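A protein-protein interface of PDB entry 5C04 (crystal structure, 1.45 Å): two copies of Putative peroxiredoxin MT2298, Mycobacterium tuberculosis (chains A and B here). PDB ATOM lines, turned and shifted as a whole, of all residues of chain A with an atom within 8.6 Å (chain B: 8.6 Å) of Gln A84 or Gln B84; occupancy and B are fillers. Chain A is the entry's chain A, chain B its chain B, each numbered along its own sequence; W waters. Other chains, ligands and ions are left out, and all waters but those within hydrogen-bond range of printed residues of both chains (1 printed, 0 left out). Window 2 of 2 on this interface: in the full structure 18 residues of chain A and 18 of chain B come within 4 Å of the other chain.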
ATOM      1  N   PHE A  42      22.163  -3.597  10.418  1.00  0.00           N
ATOM      2  CA  PHE A  42      23.100  -2.573   9.930  1.00  0.00           C
ATOM      3  C   PHE A  42      24.498  -3.137   9.779  1.00  0.00           C
ATOM      4  O   PHE A  42      25.508  -2.393   9.975  1.00  0.00           O
ATOM      5  CB  PHE A  42      23.209  -1.353  10.840  1.00  0.00           C
ATOM      6  CG  PHE A  42      21.921  -0.690  11.173  1.00  0.00           C
ATOM      7  CD1 PHE A  42      21.223   0.047  10.234  1.00  0.00           C
ATOM      8  CD2 PHE A  42      21.452  -0.725  12.488  1.00  0.00           C
ATOM      9  CE1 PHE A  42      20.039   0.712  10.595  1.00  0.00           C
ATOM     10  CE2 PHE A  42      20.276  -0.076  12.828  1.00  0.00           C
ATOM     11  CZ  PHE A  42      19.586   0.606  11.885  1.00  0.00           C
ATOM     12  N   GLN A  47      22.447  -7.338   5.871  1.00  0.00           N
ATOM     13  CA  GLN A  47      21.738  -6.461   4.937  1.00  0.00           C
ATOM     14  C   GLN A  47      21.511  -7.175   3.607  1.00  0.00           C
ATOM     15  O   GLN A  47      20.394  -7.154   3.066  1.00  0.00           O
ATOM     16  CB  GLN A  47      22.513  -5.151   4.705  1.00  0.00           C
ATOM     17  CG  GLN A  47      21.688  -4.149   3.879  1.00  0.00           C
ATOM     18  CD  GLN A  47      20.719  -3.397   4.738  1.00  0.00           C
ATOM     19  OE1 GLN A  47      21.116  -2.760   5.720  1.00  0.00           O
ATOM     20  NE2 GLN A  47      19.425  -3.500   4.431  1.00  0.00           N
ATOM     21  N   ASP A  51      17.845  -8.058   2.360  1.00  0.00           N
ATOM     22  CA  ASP A  51      17.471  -7.373   1.113  1.00  0.00           C
ATOM     23  C   ASP A  51      17.036  -8.382   0.082  1.00  0.00           C
ATOM     24  O   ASP A  51      16.050  -8.123  -0.639  1.00  0.00           O
ATOM     25  CB  ASP A  51      18.617  -6.490   0.585  1.00  0.00           C
ATOM     26  CG  ASP A  51      18.813  -5.211   1.388  1.00  0.00           C
ATOM     27  OD1 ASP A  51      18.058  -4.912   2.363  1.00  0.00           O
ATOM     28  OD2 ASP A  51      19.725  -4.423   1.016  1.00  0.00           O
ATOM     29  N   ARG A  54      13.591  -9.533   1.106  1.00  0.00           N
ATOM     30  CA  ARG A  54      12.701  -8.403   0.762  1.00  0.00           C
ATOM     31  C   ARG A  54      12.343  -8.419  -0.727  1.00  0.00           C
ATOM     32  O   ARG A  54      11.156  -8.328  -1.082  1.00  0.00           O
ATOM     33  CB  ARG A  54      13.372  -7.062   1.109  1.00  0.00           C
ATOM     34  CG  ARG A  54      12.636  -5.804   0.644  1.00  0.00           C
ATOM     35  CD  ARG A  54      13.538  -4.585   0.649  1.00  0.00           C
ATOM     36  NE  ARG A  54      14.585  -4.703  -0.364  1.00  0.00           N
ATOM     37  CZ  ARG A  54      15.702  -3.981  -0.444  1.00  0.00           C
ATOM     38  NH1 ARG A  54      16.029  -3.085   0.483  1.00  0.00           N
ATOM     39  NH2 ARG A  54      16.542  -4.208  -1.445  1.00  0.00           N
ATOM     40  N   THR A  77      15.937  -0.479  17.163  1.00  0.00           N
ATOM     41  CA  THR A  77      16.931  -0.743  16.135  1.00  0.00           C
ATOM     42  C   THR A  77      16.293  -1.310  14.881  1.00  0.00           C
ATOM     43  O   THR A  77      16.579  -0.884  13.757  1.00  0.00           O
ATOM     44  CB  THR A  77      18.002  -1.704  16.673  1.00  0.00           C
ATOM     45  OG1 THR A  77      18.736  -1.020  17.705  1.00  0.00           O
ATOM     46  CG2 THR A  77      18.970  -2.164  15.602  1.00  0.00           C
ATOM     47  N   HIS A  78      15.457  -2.325  15.098  1.00  0.00           N
ATOM     48  CA  HIS A  78      14.811  -3.004  13.984  1.00  0.00           C
ATOM     49  C   HIS A  78      13.803  -2.135  13.268  1.00  0.00           C
ATOM     50  O   HIS A  78      13.680  -2.239  12.048  1.00  0.00           O
ATOM     51  CB  HIS A  78      14.200  -4.302  14.464  1.00  0.00           C
ATOM     52  CG  HIS A  78      15.228  -5.318  14.861  1.00  0.00           C
ATOM     53  ND1 HIS A  78      14.933  -6.409  15.632  1.00  0.00           N
ATOM     54  CD2 HIS A  78      16.563  -5.379  14.617  1.00  0.00           C
ATOM     55  CE1 HIS A  78      16.029  -7.125  15.827  1.00  0.00           C
ATOM     56  NE2 HIS A  78      17.036  -6.517  15.230  1.00  0.00           N
ATOM     57  N   LYS A  79      13.142  -1.232  13.994  1.00  0.00           N
ATOM     58  CA  LYS A  79      12.224  -0.298  13.352  1.00  0.00           C
ATOM     59  C   LYS A  79      12.924   0.632  12.367  1.00  0.00           C
ATOM     60  O   LYS A  79      12.480   0.791  11.208  1.00  0.00           O
ATOM     61  CB  LYS A  79      11.441   0.514  14.388  1.00  0.00           C
ATOM     62  CG  LYS A  79      10.422   1.486  13.783  1.00  0.00           C
ATOM     63  CD  LYS A  79       9.417   0.783  12.882  1.00  0.00           C
ATOM     64  CE  LYS A  79       8.258   1.688  12.502  1.00  0.00           C
ATOM     65  NZ  LYS A  79       7.351   1.013  11.532  1.00  0.00           N
ATOM     66  N   ILE A  80      14.018   1.260  12.783  1.00  0.00           N
ATOM     67  CA  ILE A  80      14.776   2.137  11.897  1.00  0.00           C
ATOM     68  C   ILE A  80      15.357   1.350  10.707  1.00  0.00           C
ATOM     69  O   ILE A  80      15.334   1.767   9.551  1.00  0.00           O
ATOM     70  CB  ILE A  80      15.898   2.877  12.668  1.00  0.00           C
ATOM     71  CG1 ILE A  80      15.305   3.824  13.722  1.00  0.00           C
ATOM     72  CG2 ILE A  80      16.822   3.598  11.701  1.00  0.00           C
ATOM     73  CD1 ILE A  80      14.418   4.925  13.183  1.00  0.00           C
ATOM     74  N   TRP A  81      15.925   0.179  10.991  1.00  0.00           N
ATOM     75  CA  TRP A  81      16.537  -0.632   9.949  1.00  0.00           C
ATOM     76  C   TRP A  81      15.476  -1.032   8.916  1.00  0.00           C
ATOM     77  O   TRP A  81      15.701  -0.926   7.705  1.00  0.00           O
ATOM     78  CB  TRP A  81      17.191  -1.866  10.556  1.00  0.00           C
ATOM     79  CG  TRP A  81      18.125  -2.588   9.622  1.00  0.00           C
ATOM     80  CD1 TRP A  81      18.928  -2.045   8.662  1.00  0.00           C
ATOM     81  CD2 TRP A  81      18.351  -4.004   9.571  1.00  0.00           C
ATOM     82  NE1 TRP A  81      19.654  -3.025   8.028  1.00  0.00           N
ATOM     83  CE2 TRP A  81      19.320  -4.241   8.569  1.00  0.00           C
ATOM     84  CE3 TRP A  81      17.850  -5.074  10.290  1.00  0.00           C
ATOM     85  CZ2 TRP A  81      19.781  -5.516   8.267  1.00  0.00           C
ATOM     86  CZ3 TRP A  81      18.303  -6.355   9.984  1.00  0.00           C
ATOM     87  CH2 TRP A  81      19.258  -6.562   8.979  1.00  0.00           C
ATOM     88  N   ALA A  82      14.313  -1.460   9.409  1.00  0.00           N
ATOM     89  CA  ALA A  82      13.221  -1.868   8.525  1.00  0.00           C
ATOM     90  C   ALA A  82      12.676  -0.705   7.713  1.00  0.00           C
ATOM     91  O   ALA A  82      12.433  -0.861   6.492  1.00  0.00           O
ATOM     92  CB  ALA A  82      12.087  -2.498   9.317  1.00  0.00           C
ATOM     93  N   THR A  83      12.511   0.445   8.346  1.00  0.00           N
ATOM     94  CA  THR A  83      12.036   1.632   7.616  1.00  0.00           C
ATOM     95  C   THR A  83      13.017   2.046   6.521  1.00  0.00           C
ATOM     96  O   THR A  83      12.627   2.267   5.366  1.00  0.00           O
ATOM     97  CB  THR A  83      11.762   2.798   8.567  1.00  0.00           C
ATOM     98  OG1 THR A  83      10.741   2.403   9.478  1.00  0.00           O
ATOM     99  CG2 THR A  83      11.337   4.040   7.781  1.00  0.00           C
ATOM    100  N   GLN A  84      14.300   2.140   6.854  1.00  0.00           N
ATOM    101  CA  GLN A  84      15.289   2.569   5.885  1.00  0.00           C
ATOM    102  C   GLN A  84      15.531   1.531   4.775  1.00  0.00           C
ATOM    103  O   GLN A  84      15.923   1.877   3.650  1.00  0.00           O
ATOM    104  CB  GLN A  84      16.574   2.967   6.629  1.00  0.00           C
ATOM    105  CG  GLN A  84      16.354   4.189   7.511  1.00  0.00           C
ATOM    106  CD  GLN A  84      17.595   4.679   8.235  1.00  0.00           C
ATOM    107  OE1 GLN A  84      18.707   4.182   8.028  1.00  0.00           O
ATOM    108  NE2 GLN A  84      17.408   5.694   9.070  1.00  0.00           N
ATOM    109  N   SER A  85      15.288   0.250   5.064  1.00  0.00           N
ATOM    110  CA  SER A  85      15.533  -0.831   4.111  1.00  0.00           C
ATOM    111  C   SER A  85      14.280  -1.268   3.345  1.00  0.00           C
ATOM    112  O   SER A  85      14.388  -2.111   2.430  1.00  0.00           O
ATOM    113  CB  SER A  85      16.097  -2.069   4.824  1.00  0.00           C
ATOM    114  OG  SER A  85      17.267  -1.735   5.576  1.00  0.00           O
ATOM    115  N   GLY A  86      13.119  -0.769   3.760  1.00  0.00           N
ATOM    116  CA  GLY A  86      11.863  -1.197   3.178  1.00  0.00           C
ATOM    117  C   GLY A  86      11.459  -2.607   3.531  1.00  0.00           C
ATOM    118  O   GLY A  86      10.839  -3.318   2.679  1.00  0.00           O
ATOM    119  N   PHE A  87      11.765  -3.043   4.763  1.00  0.00           N
ATOM    120  CA  PHE A  87      11.356  -4.376   5.218  1.00  0.00           C
ATOM    121  C   PHE A  87       9.944  -4.260   5.795  1.00  0.00           C
ATOM    122  O   PHE A  87       9.716  -3.480   6.736  1.00  0.00           O
ATOM    123  CB  PHE A  87      12.285  -4.921   6.327  1.00  0.00           C
ATOM    124  CG  PHE A  87      13.727  -5.084   5.946  1.00  0.00           C
ATOM    125  CD1 PHE A  87      14.135  -5.321   4.644  1.00  0.00           C
ATOM    126  CD2 PHE A  87      14.691  -5.009   6.936  1.00  0.00           C
ATOM    127  CE1 PHE A  87      15.473  -5.504   4.344  1.00  0.00           C
ATOM    128  CE2 PHE A  87      16.030  -5.199   6.635  1.00  0.00           C
ATOM    129  CZ  PHE A  87      16.415  -5.435   5.347  1.00  0.00           C
ATOM    130  N   PHE B  42      18.184   5.316  18.929  1.00  0.00           N
ATOM    131  CA  PHE B  42      16.974   5.480  18.109  1.00  0.00           C
ATOM    132  C   PHE B  42      15.681   5.551  18.912  1.00  0.00           C
ATOM    133  O   PHE B  42      14.615   5.108  18.397  1.00  0.00           O
ATOM    134  CB  PHE B  42      16.811   4.367  17.085  1.00  0.00           C
ATOM    135  CG  PHE B  42      18.008   4.128  16.213  1.00  0.00           C
ATOM    136  CD1 PHE B  42      18.394   5.045  15.258  1.00  0.00           C
ATOM    137  CD2 PHE B  42      18.676   2.910  16.280  1.00  0.00           C
ATOM    138  CE1 PHE B  42      19.478   4.767  14.402  1.00  0.00           C
ATOM    139  CE2 PHE B  42      19.754   2.655  15.450  1.00  0.00           C
ATOM    140  CZ  PHE B  42      20.158   3.586  14.555  1.00  0.00           C
ATOM    141  N   GLN B  47      17.587  10.261  22.027  1.00  0.00           N
ATOM    142  CA  GLN B  47      17.940  11.139  20.906  1.00  0.00           C
ATOM    143  C   GLN B  47      18.009  12.580  21.394  1.00  0.00           C
ATOM    144  O   GLN B  47      18.956  13.311  21.068  1.00  0.00           O
ATOM    145  CB  GLN B  47      16.890  11.067  19.819  1.00  0.00           C
ATOM    146  CG  GLN B  47      17.277  11.835  18.563  1.00  0.00           C
ATOM    147  CD  GLN B  47      18.247  11.054  17.717  1.00  0.00           C
ATOM    148  OE1 GLN B  47      17.951   9.919  17.309  1.00  0.00           O
ATOM    149  NE2 GLN B  47      19.410  11.629  17.452  1.00  0.00           N
ATOM    150  N   ASP B  51      21.452  14.587  21.396  1.00  0.00           N
ATOM    151  CA  ASP B  51      21.378  15.792  20.508  1.00  0.00           C
ATOM    152  C   ASP B  51      21.800  17.028  21.280  1.00  0.00           C
ATOM    153  O   ASP B  51      22.523  17.889  20.748  1.00  0.00           O
ATOM    154  CB  ASP B  51      19.961  15.987  19.983  1.00  0.00           C
ATOM    155  CG  ASP B  51      19.602  15.062  18.831  1.00  0.00           C
ATOM    156  OD1 ASP B  51      20.459  14.245  18.412  1.00  0.00           O
ATOM    157  OD2 ASP B  51      18.460  15.185  18.317  1.00  0.00           O
ATOM    158  N   ARG B  54      25.575  16.837  21.815  1.00  0.00           N
ATOM    159  CA  ARG B  54      26.155  17.187  20.507  1.00  0.00           C
ATOM    160  C   ARG B  54      26.157  18.691  20.295  1.00  0.00           C
ATOM    161  O   ARG B  54      27.148  19.275  19.829  1.00  0.00           O
ATOM    162  CB  ARG B  54      25.335  16.538  19.404  1.00  0.00           C
ATOM    163  CG  ARG B  54      25.678  16.897  17.945  1.00  0.00           C
ATOM    164  CD  ARG B  54      24.551  16.481  17.022  1.00  0.00           C
ATOM    165  NE  ARG B  54      23.370  17.295  17.276  1.00  0.00           N
ATOM    166  CZ  ARG B  54      22.152  17.067  16.816  1.00  0.00           C
ATOM    167  NH1 ARG B  54      21.883  16.003  16.079  1.00  0.00           N
ATOM    168  NH2 ARG B  54      21.168  17.881  17.153  1.00  0.00           N
ATOM    169  N   THR B  77      25.062  -0.571  15.463  1.00  0.00           N
ATOM    170  CA  THR B  77      23.919   0.269  15.796  1.00  0.00           C
ATOM    171  C   THR B  77      24.372   1.675  16.119  1.00  0.00           C
ATOM    172  O   THR B  77      23.799   2.668  15.623  1.00  0.00           O
ATOM    173  CB  THR B  77      23.149  -0.324  16.993  1.00  0.00           C
ATOM    174  OG1 THR B  77      22.538  -1.540  16.568  1.00  0.00           O
ATOM    175  CG2 THR B  77      22.043   0.596  17.540  1.00  0.00           C
ATOM    176  N   HIS B  78      25.365   1.756  16.992  1.00  0.00           N
ATOM    177  CA  HIS B  78      25.912   3.064  17.390  1.00  0.00           C
ATOM    178  C   HIS B  78      26.534   3.809  16.214  1.00  0.00           C
ATOM    179  O   HIS B  78      26.450   5.035  16.124  1.00  0.00           O
ATOM    180  CB  HIS B  78      26.829   2.930  18.564  1.00  0.00           C
ATOM    181  CG  HIS B  78      26.113   2.527  19.824  1.00  0.00           C
ATOM    182  ND1 HIS B  78      26.749   1.989  20.908  1.00  0.00           N
ATOM    183  CD2 HIS B  78      24.789   2.546  20.125  1.00  0.00           C
ATOM    184  CE1 HIS B  78      25.862   1.752  21.857  1.00  0.00           C
ATOM    185  NE2 HIS B  78      24.660   2.038  21.392  1.00  0.00           N
ATOM    186  N   LYS B  79      27.172   3.079  15.307  1.00  0.00           N
ATOM    187  CA  LYS B  79      27.795   3.746  14.145  1.00  0.00           C
ATOM    188  C   LYS B  79      26.744   4.426  13.274  1.00  0.00           C
ATOM    189  O   LYS B  79      26.925   5.581  12.880  1.00  0.00           O
ATOM    190  CB  LYS B  79      28.661   2.792  13.329  1.00  0.00           C
ATOM    191  CG  LYS B  79      29.374   3.429  12.138  1.00  0.00           C
ATOM    192  CD  LYS B  79      30.456   4.407  12.562  1.00  0.00           C
ATOM    193  CE  LYS B  79      31.191   4.908  11.339  1.00  0.00           C
ATOM    194  NZ  LYS B  79      32.193   5.953  11.712  1.00  0.00           N
ATOM    195  N   ILE B  80      25.661   3.726  12.929  1.00  0.00           N
ATOM    196  CA  ILE B  80      24.583   4.280  12.098  1.00  0.00           C
ATOM    197  C   ILE B  80      23.958   5.474  12.826  1.00  0.00           C
ATOM    198  O   ILE B  80      23.733   6.538  12.270  1.00  0.00           O
ATOM    199  CB  ILE B  80      23.502   3.208  11.791  1.00  0.00           C
ATOM    200  CG1 ILE B  80      24.069   2.139  10.850  1.00  0.00           C
ATOM    201  CG2 ILE B  80      22.258   3.836  11.171  1.00  0.00           C
ATOM    202  CD1 ILE B  80      24.082   2.549   9.401  1.00  0.00           C
ATOM    203  N   TRP B  81      23.654   5.268  14.097  1.00  0.00           N
ATOM    204  CA  TRP B  81      23.005   6.314  14.885  1.00  0.00           C
ATOM    205  C   TRP B  81      23.880   7.556  14.970  1.00  0.00           C
ATOM    206  O   TRP B  81      23.388   8.696  14.752  1.00  0.00           O
ATOM    207  CB  TRP B  81      22.679   5.794  16.279  1.00  0.00           C
ATOM    208  CG  TRP B  81      21.706   6.674  17.055  1.00  0.00           C
ATOM    209  CD1 TRP B  81      20.638   7.353  16.578  1.00  0.00           C
ATOM    210  CD2 TRP B  81      21.714   6.877  18.466  1.00  0.00           C
ATOM    211  NE1 TRP B  81      19.978   7.993  17.607  1.00  0.00           N
ATOM    212  CE2 TRP B  81      20.626   7.715  18.777  1.00  0.00           C
ATOM    213  CE3 TRP B  81      22.553   6.455  19.490  1.00  0.00           C
ATOM    214  CZ2 TRP B  81      20.356   8.110  20.075  1.00  0.00           C
ATOM    215  CZ3 TRP B  81      22.281   6.848  20.766  1.00  0.00           C
ATOM    216  CH2 TRP B  81      21.189   7.681  21.043  1.00  0.00           C
ATOM    217  N   ALA B  82      25.177   7.366  15.225  1.00  0.00           N
ATOM    218  CA  ALA B  82      26.110   8.509  15.319  1.00  0.00           C
ATOM    219  C   ALA B  82      26.295   9.198  13.991  1.00  0.00           C
ATOM    220  O   ALA B  82      26.351  10.431  13.926  1.00  0.00           O
ATOM    221  CB  ALA B  82      27.454   8.047  15.827  1.00  0.00           C
ATOM    222  N   THR B  83      26.453   8.440  12.924  1.00  0.00           N
ATOM    223  CA  THR B  83      26.672   9.047  11.606  1.00  0.00           C
ATOM    224  C   THR B  83      25.431   9.846  11.208  1.00  0.00           C
ATOM    225  O   THR B  83      25.544  11.011  10.791  1.00  0.00           O
ATOM    226  CB  THR B  83      27.025   8.007  10.512  1.00  0.00           C
ATOM    227  OG1 THR B  83      26.027   6.989  10.443  1.00  0.00           O
ATOM    228  CG2 THR B  83      28.361   7.372  10.769  1.00  0.00           C
ATOM    229  N   GLN B  84      24.250   9.261  11.357  1.00  0.00           N
ATOM    230  CA  GLN B  84      22.990   9.937  10.978  1.00  0.00           C
ATOM    231  C   GLN B  84      22.661  11.152  11.849  1.00  0.00           C
ATOM    232  O   GLN B  84      22.021  12.118  11.391  1.00  0.00           O
ATOM    233  CB  GLN B  84      21.818   8.964  10.947  1.00  0.00           C
ATOM    234  CG  GLN B  84      21.914   7.962   9.807  1.00  0.00           C
ATOM    235  CD  GLN B  84      20.729   7.007   9.660  1.00  0.00           C
ATOM    236  OE1 GLN B  84      19.744   7.032  10.412  1.00  0.00           O
ATOM    237  NE2 GLN B  84      20.879   6.082   8.714  1.00  0.00           N
ATOM    238  N   SER B  85      23.090  11.128  13.107  1.00  0.00           N
ATOM    239  CA  SER B  85      22.797  12.222  14.041  1.00  0.00           C
ATOM    240  C   SER B  85      23.908  13.240  14.164  1.00  0.00           C
ATOM    241  O   SER B  85      23.728  14.258  14.852  1.00  0.00           O
ATOM    242  CB  SER B  85      22.554  11.640  15.454  1.00  0.00           C
ATOM    243  OG  SER B  85      21.540  10.673  15.479  1.00  0.00           O
ATOM    244  N   GLY B  86      25.078  12.979  13.586  1.00  0.00           N
ATOM    245  CA  GLY B  86      26.238  13.868  13.772  1.00  0.00           C
ATOM    246  C   GLY B  86      26.889  13.804  15.139  1.00  0.00           C
ATOM    247  O   GLY B  86      27.455  14.784  15.641  1.00  0.00           O
ATOM    248  N   PHE B  87      26.819  12.642  15.797  1.00  0.00           N
ATOM    249  CA  PHE B  87      27.544  12.455  17.034  1.00  0.00           C
ATOM    250  C   PHE B  87      29.003  12.113  16.751  1.00  0.00           C
ATOM    251  O   PHE B  87      29.280  11.155  16.029  1.00  0.00           O
ATOM    252  CB  PHE B  87      26.967  11.317  17.861  1.00  0.00           C
ATOM    253  CG  PHE B  87      25.502  11.428  18.197  1.00  0.00           C
ATOM    254  CD1 PHE B  87      24.868  12.661  18.342  1.00  0.00           C
ATOM    255  CD2 PHE B  87      24.746  10.265  18.434  1.00  0.00           C
ATOM    256  CE1 PHE B  87      23.545  12.755  18.702  1.00  0.00           C
ATOM    257  CE2 PHE B  87      23.409  10.365  18.792  1.00  0.00           C
ATOM    258  CZ  PHE B  87      22.799  11.601  18.900  1.00  0.00           C
HETATM  259  O   HOH W   1      20.835  -2.615  18.401  1.00  0.00           O
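Gln A84 touches just one residue of chain B: Gln B84 (3.0 Å).
Of the printed residues of chain A, Gln B84 touches Gln A84 (3.0 Å).
No residue of chain B comes within 4 Å of Thr A83.
No residue of chain B comes within 4 Å of Ser A85.
No residue of chain A comes within 4 Å of Ser B85.
Printed residues of chain B within 4 Å of Thr A77: Thr B77 (3.7 Å).
Of the printed residues of chain A, Ile B80 touches Phe A42.
The nearest printed residue of chain A that does not touch Gln B84 is Ile A80 (4.7 Å).
The nearest printed residue of chain A that does not touch Ile B80 is Gln A84 (4.8 Å).
Phe B42 touches its own counterpart, Phe A42.
Phe A42 touches Ile B80, and with the chains exchanged Ile A80 touches Phe B42.
Thr A77 touches its own counterpart, Thr B77.
Gln A84 touches its own counterpart, Gln B84.
15 positions are printed for both chains.
Of the 15 printed residues of chain B, 4 touch a printed residue of chain A.
Printed residues of chain B that touch a printed residue of chain A: Phe B42, Thr B77, Ile B80 and Gln B84.
Hydrophobic or aromatic side chains of chain B that line the printed part of chain A: Phe B42 and Ile B80.
Printed residues of chain A that touch a printed residue of chain B: Phe A42, Thr A77, Ile A80 and Gln A84.
Hydrophobic or aromatic side chains of chain A within 4 Å of the printed part of chain B: Phe A42 and Ile A80.
Among the printed residues, no Asp or Glu carboxylate lies within 4 Å of a Lys or Arg side-chain nitrogen of the other chain.
Water W1 lies within hydrogen-bond range of OG1 of Thr B77 (2.7 Å) and OG1 of Thr A77 (2.7 Å).
O of Ile B80 lies within hydrogen-bond range of OG1 of Thr B83, 3.0 Å away.
OE1 of Gln A84 lies within hydrogen-bond range of NE2 of Gln B84 (3.0 Å).
Among the printed residues, merely in contact across the chains: Phe A42 with Ile B80 (3.6 Å), Ile A80 with Phe B42 (3.7 Å), Thr A77 with Thr B77 (3.7 Å) and Phe A42 with Phe B42 (3.8 Å).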
